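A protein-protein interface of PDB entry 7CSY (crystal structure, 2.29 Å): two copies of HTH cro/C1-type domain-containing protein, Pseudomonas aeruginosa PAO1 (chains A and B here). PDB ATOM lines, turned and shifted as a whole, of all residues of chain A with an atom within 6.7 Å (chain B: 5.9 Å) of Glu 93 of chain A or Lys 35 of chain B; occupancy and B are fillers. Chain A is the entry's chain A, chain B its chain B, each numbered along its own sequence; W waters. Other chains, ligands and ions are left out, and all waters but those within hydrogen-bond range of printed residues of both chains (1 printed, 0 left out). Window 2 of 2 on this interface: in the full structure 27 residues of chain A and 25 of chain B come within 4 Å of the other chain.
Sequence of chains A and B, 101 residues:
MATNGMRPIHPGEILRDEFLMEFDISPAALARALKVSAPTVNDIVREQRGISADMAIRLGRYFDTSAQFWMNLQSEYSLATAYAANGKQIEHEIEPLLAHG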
ATOM      1  N   LYS A  88      -8.377  12.218 -12.469  1.00  0.00           N
ATOM      2  CA  LYS A  88      -7.965  12.944 -13.667  1.00  0.00           C
ATOM      3  C   LYS A  88      -7.175  14.198 -13.311  1.00  0.00           C
ATOM      4  O   LYS A  88      -6.135  14.480 -13.918  1.00  0.00           O
ATOM      5  CB  LYS A  88      -9.191  13.296 -14.507  1.00  0.00           C
ATOM      6  CG  LYS A  88      -9.605  12.205 -15.484  1.00  0.00           C
ATOM      7  CD  LYS A  88      -8.545  12.030 -16.570  1.00  0.00           C
ATOM      8  CE  LYS A  88      -8.887  10.879 -17.508  1.00  0.00           C
ATOM      9  NZ  LYS A  88      -7.755  10.532 -18.408  1.00  0.00           N
ATOM     10  N   GLN A  89      -7.647  14.958 -12.319  1.00  0.00           N
ATOM     11  CA  GLN A  89      -6.920  16.142 -11.879  1.00  0.00           C
ATOM     12  C   GLN A  89      -5.568  15.772 -11.281  1.00  0.00           C
ATOM     13  O   GLN A  89      -4.562  16.432 -11.558  1.00  0.00           O
ATOM     14  CB  GLN A  89      -7.766  16.919 -10.872  1.00  0.00           C
ATOM     15  CG  GLN A  89      -6.982  17.918 -10.034  1.00  0.00           C
ATOM     16  CD  GLN A  89      -6.363  19.025 -10.873  1.00  0.00           C
ATOM     17  OE1 GLN A  89      -7.030  19.632 -11.713  1.00  0.00           O
ATOM     18  NE2 GLN A  89      -5.076  19.287 -10.655  1.00  0.00           N
ATOM     19  N   ILE A  90      -5.521  14.712 -10.468  1.00  0.00           N
ATOM     20  CA  ILE A  90      -4.265  14.310  -9.835  1.00  0.00           C
ATOM     21  C   ILE A  90      -3.248  13.883 -10.881  1.00  0.00           C
ATOM     22  O   ILE A  90      -2.049  14.171 -10.756  1.00  0.00           O
ATOM     23  CB  ILE A  90      -4.514  13.187  -8.814  1.00  0.00           C
ATOM     24  CG1 ILE A  90      -5.088  13.750  -7.517  1.00  0.00           C
ATOM     25  CG2 ILE A  90      -3.224  12.425  -8.541  1.00  0.00           C
ATOM     26  CD1 ILE A  90      -5.334  12.688  -6.479  1.00  0.00           C
ATOM     27  N   GLU A  91      -3.700  13.168 -11.917  1.00  0.00           N
ATOM     28  CA  GLU A  91      -2.790  12.788 -12.993  1.00  0.00           C
ATOM     29  C   GLU A  91      -2.279  14.015 -13.741  1.00  0.00           C
ATOM     30  O   GLU A  91      -1.118  14.054 -14.170  1.00  0.00           O
ATOM     31  CB  GLU A  91      -3.480  11.821 -13.958  1.00  0.00           C
ATOM     32  CG  GLU A  91      -3.595  10.404 -13.443  1.00  0.00           C
ATOM     33  CD  GLU A  91      -4.633   9.579 -14.196  1.00  0.00           C
ATOM     34  OE1 GLU A  91      -5.152  10.024 -15.259  1.00  0.00           O
ATOM     35  OE2 GLU A  91      -4.949   8.479 -13.696  1.00  0.00           O
ATOM     36  N   HIS A  92      -3.140  15.022 -13.915  1.00  0.00           N
ATOM     37  CA  HIS A  92      -2.729  16.255 -14.577  1.00  0.00           C
ATOM     38  C   HIS A  92      -1.656  17.002 -13.772  1.00  0.00           C
ATOM     39  O   HIS A  92      -0.747  17.603 -14.352  1.00  0.00           O
ATOM     40  CB  HIS A  92      -3.959  17.137 -14.812  1.00  0.00           C
ATOM     41  CG  HIS A  92      -3.664  18.445 -15.490  1.00  0.00           C
ATOM     42  ND1 HIS A  92      -2.990  19.477 -14.868  1.00  0.00           N
ATOM     43  CD2 HIS A  92      -3.975  18.895 -16.732  1.00  0.00           C
ATOM     44  CE1 HIS A  92      -2.885  20.498 -15.701  1.00  0.00           C
ATOM     45  NE2 HIS A  92      -3.476  20.172 -16.838  1.00  0.00           N
ATOM     46  N   GLU A  93      -1.740  16.984 -12.444  1.00  0.00           N
ATOM     47  CA  GLU A  93      -0.873  17.830 -11.636  1.00  0.00           C
ATOM     48  C   GLU A  93       0.363  17.115 -11.102  1.00  0.00           C
ATOM     49  O   GLU A  93       1.225  17.767 -10.518  1.00  0.00           O
ATOM     50  CB  GLU A  93      -1.665  18.462 -10.480  1.00  0.00           C
ATOM     51  CG  GLU A  93      -2.321  17.509  -9.500  1.00  0.00           C
ATOM     52  CD  GLU A  93      -3.156  18.241  -8.457  1.00  0.00           C
ATOM     53  OE1 GLU A  93      -3.773  19.259  -8.811  1.00  0.00           O
ATOM     54  OE2 GLU A  93      -3.196  17.812  -7.287  1.00  0.00           O
ATOM     55  N   ILE A  94       0.496  15.809 -11.311  1.00  0.00           N
ATOM     56  CA  ILE A  94       1.673  15.071 -10.868  1.00  0.00           C
ATOM     57  C   ILE A  94       2.290  14.354 -12.065  1.00  0.00           C
ATOM     58  O   ILE A  94       1.609  13.581 -12.751  1.00  0.00           O
ATOM     59  CB  ILE A  94       1.345  14.060  -9.762  1.00  0.00           C
ATOM     60  CG1 ILE A  94       0.774  14.754  -8.532  1.00  0.00           C
ATOM     61  CG2 ILE A  94       2.583  13.268  -9.392  1.00  0.00           C
ATOM     62  CD1 ILE A  94       0.298  13.770  -7.485  1.00  0.00           C
ATOM     63  N   GLU A  95       3.584  14.606 -12.313  1.00  0.00           N
ATOM     64  CA  GLU A  95       4.326  13.806 -13.277  1.00  0.00           C
ATOM     65  C   GLU A  95       5.095  12.723 -12.548  1.00  0.00           C
ATOM     66  O   GLU A  95       5.762  13.013 -11.547  1.00  0.00           O
ATOM     67  CB  GLU A  95       5.285  14.664 -14.100  1.00  0.00           C
ATOM     68  CG  GLU A  95       4.578  15.855 -14.758  1.00  0.00           C
ATOM     69  CD  GLU A  95       3.745  15.449 -15.983  1.00  0.00           C
ATOM     70  OE1 GLU A  95       2.517  15.206 -15.829  1.00  0.00           O
ATOM     71  OE2 GLU A  95       4.314  15.387 -17.099  1.00  0.00           O
ATOM     72  N   LEU B  30       8.931  15.898  -1.577  1.00  0.00           N
ATOM     73  CA  LEU B  30       7.819  15.049  -1.989  1.00  0.00           C
ATOM     74  C   LEU B  30       6.509  15.834  -1.987  1.00  0.00           C
ATOM     75  O   LEU B  30       5.695  15.686  -2.907  1.00  0.00           O
ATOM     76  CB  LEU B  30       7.708  13.811  -1.090  1.00  0.00           C
ATOM     77  CG  LEU B  30       6.552  12.876  -1.526  1.00  0.00           C
ATOM     78  CD1 LEU B  30       6.727  12.399  -2.969  1.00  0.00           C
ATOM     79  CD2 LEU B  30       6.362  11.679  -0.596  1.00  0.00           C
ATOM     80  N   ALA B  31       6.311  16.707  -0.987  1.00  0.00           N
ATOM     81  CA  ALA B  31       5.079  17.493  -0.930  1.00  0.00           C
ATOM     82  C   ALA B  31       4.950  18.390  -2.146  1.00  0.00           C
ATOM     83  O   ALA B  31       3.883  18.456  -2.767  1.00  0.00           O
ATOM     84  CB  ALA B  31       5.028  18.327   0.346  1.00  0.00           C
ATOM     85  N   ARG B  32       6.041  19.060  -2.531  1.00  0.00           N
ATOM     86  CA  ARG B  32       6.011  19.869  -3.751  1.00  0.00           C
ATOM     87  C   ARG B  32       5.669  19.015  -4.972  1.00  0.00           C
ATOM     88  O   ARG B  32       4.875  19.436  -5.825  1.00  0.00           O
ATOM     89  CB  ARG B  32       7.348  20.594  -3.950  1.00  0.00           C
ATOM     90  CG  ARG B  32       7.528  21.849  -3.085  1.00  0.00           C
ATOM     91  CD  ARG B  32       8.744  22.688  -3.507  1.00  0.00           C
ATOM     92  NE  ARG B  32      10.034  22.062  -3.195  1.00  0.00           N
ATOM     93  CZ  ARG B  32      10.555  21.979  -1.970  1.00  0.00           C
ATOM     94  NH1 ARG B  32       9.893  22.470  -0.929  1.00  0.00           N
ATOM     95  NH2 ARG B  32      11.735  21.390  -1.775  1.00  0.00           N
ATOM     96  N   ALA B  33       6.238  17.800  -5.061  1.00  0.00           N
ATOM     97  CA  ALA B  33       5.946  16.928  -6.203  1.00  0.00           C
ATOM     98  C   ALA B  33       4.487  16.459  -6.208  1.00  0.00           C
ATOM     99  O   ALA B  33       3.861  16.393  -7.272  1.00  0.00           O
ATOM    100  CB  ALA B  33       6.886  15.725  -6.205  1.00  0.00           C
ATOM    101  N   LEU B  34       3.931  16.121  -5.033  1.00  0.00           N
ATOM    102  CA  LEU B  34       2.566  15.607  -4.945  1.00  0.00           C
ATOM    103  C   LEU B  34       1.498  16.705  -4.994  1.00  0.00           C
ATOM    104  O   LEU B  34       0.313  16.373  -5.028  1.00  0.00           O
ATOM    105  CB  LEU B  34       2.390  14.791  -3.657  1.00  0.00           C
ATOM    106  CG  LEU B  34       3.273  13.575  -3.349  1.00  0.00           C
ATOM    107  CD1 LEU B  34       2.753  12.843  -2.088  1.00  0.00           C
ATOM    108  CD2 LEU B  34       3.378  12.642  -4.535  1.00  0.00           C
ATOM    109  N   LYS B  35       1.891  17.986  -4.991  1.00  0.00           N
ATOM    110  CA  LYS B  35       0.982  19.137  -4.871  1.00  0.00           C
ATOM    111  C   LYS B  35       0.121  19.073  -3.604  1.00  0.00           C
ATOM    112  O   LYS B  35      -1.077  19.370  -3.631  1.00  0.00           O
ATOM    113  CB  LYS B  35       0.095  19.303  -6.111  1.00  0.00           C
ATOM    114  CG  LYS B  35       0.840  19.295  -7.434  1.00  0.00           C
ATOM    115  CD  LYS B  35       2.029  20.261  -7.439  1.00  0.00           C
ATOM    116  CE  LYS B  35       2.750  20.245  -8.785  1.00  0.00           C
ATOM    117  NZ  LYS B  35       1.879  20.774  -9.894  1.00  0.00           N
ATOM    118  N   VAL B  36       0.724  18.703  -2.478  1.00  0.00           N
ATOM    119  CA  VAL B  36       0.041  18.795  -1.194  1.00  0.00           C
ATOM    120  C   VAL B  36       0.914  19.605  -0.242  1.00  0.00           C
ATOM    121  O   VAL B  36       2.115  19.773  -0.452  1.00  0.00           O
ATOM    122  CB  VAL B  36      -0.309  17.410  -0.587  1.00  0.00           C
ATOM    123  CG1 VAL B  36      -1.246  16.639  -1.522  1.00  0.00           C
ATOM    124  CG2 VAL B  36       0.937  16.586  -0.287  1.00  0.00           C
ATOM    125  N   SER B  37       0.288  20.127   0.807  1.00  0.00           N
ATOM    126  CA  SER B  37       1.025  20.896   1.803  1.00  0.00           C
ATOM    127  C   SER B  37       2.073  20.030   2.495  1.00  0.00           C
ATOM    128  O   SER B  37       1.898  18.821   2.679  1.00  0.00           O
ATOM    129  CB  SER B  37       0.071  21.481   2.841  1.00  0.00           C
ATOM    130  OG  SER B  37      -0.508  20.445   3.623  1.00  0.00           O
ATOM    131  N   ARG B  58      -1.980   9.870  -5.251  1.00  0.00           N
ATOM    132  CA  ARG B  58      -0.778  10.671  -5.487  1.00  0.00           C
ATOM    133  C   ARG B  58       0.482   9.817  -5.381  1.00  0.00           C
ATOM    134  O   ARG B  58       1.344   9.847  -6.264  1.00  0.00           O
ATOM    135  CB  ARG B  58      -0.734  11.833  -4.500  1.00  0.00           C
ATOM    136  CG  ARG B  58      -1.831  12.833  -4.746  1.00  0.00           C
ATOM    137  CD  ARG B  58      -1.857  13.967  -3.745  1.00  0.00           C
ATOM    138  NE  ARG B  58      -3.126  14.639  -3.901  1.00  0.00           N
ATOM    139  CZ  ARG B  58      -3.341  15.640  -4.740  1.00  0.00           C
ATOM    140  NH1 ARG B  58      -2.354  16.121  -5.465  1.00  0.00           N
ATOM    141  NH2 ARG B  58      -4.554  16.155  -4.854  1.00  0.00           N
HETATM  142  O   HOH W   1      -3.322  20.214  -5.635  1.00  0.00           O
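NZ of Lys 35 of chain B lies within hydrogen-bond range of O of Glu 93 of chain A (3.1 Å).
The guanidinium group (NH1) of Arg 58 of chain B is in salt-bridge range of the side-chain carboxylate (OE2) of Glu 93 of chain A (2.6 Å).
The backbone carbonyl oxygen (O) of Leu 34 of chain B sits at hydrogen-bond distance from the guanidinium group (NH1) of Arg 58 of chain B, at 2.7 Å.
Hydrophobic or aromatic side chains of chain A that line the printed part of chain B: Ile 90 and Ile 94.
Among the printed residues, Asp or Glu carboxylates within 4 Å of a Lys or Arg side-chain nitrogen of the other chain: Glu 93 of chain A with Arg 58 of chain B.
Water W1 bridges OE2 of Glu 93 of chain A (2.9 Å) and O of Lys 35 of chain B (3.1 Å).
No position is printed for both chains.
Of the 6 pairs that touch across the chains among the printed residues, none has its exchanged pair printed and touching as well.
Among the printed residues, pairs that only touch across the chains: Ile 90 of chain A with Arg 58 of chain B (3.6 Å), Ile 94 of chain A with Ala 33 of chain B (3.7 Å), Ile 94 of chain A with Leu 34 of chain B (3.6 Å) and Ile 94 of chain A with Arg 58 of chain B (3.6 Å).
Glu 93 of chain A touches two residues of chain B.
Of chain A, only Glu 93 (3.1 Å) comes within 4 Å of Lys 35 of chain B.
Printed residues of chain A within 4 Å of Leu 34 of chain B: Ile 94 (3.6 Å).
Of the printed residues of chain B, Ile 90 of chain A touches Arg 58.
Printed residues of chain A within 4 Å of Arg 58 of chain B: Ile 90, Glu 93 and Ile 94.
Of the printed residues of chain B, Ile 94 of chain A touches Ala 33, Leu 34 and Arg 58.
Lys 88 of chain A touches none of the printed residues of chain B.
Ala 31 of chain B touches none of the printed residues of chain A.
The nearest printed residue of chain B that does not touch Glu 93 of chain A is Ala 33 of chain B (4.4 Å).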
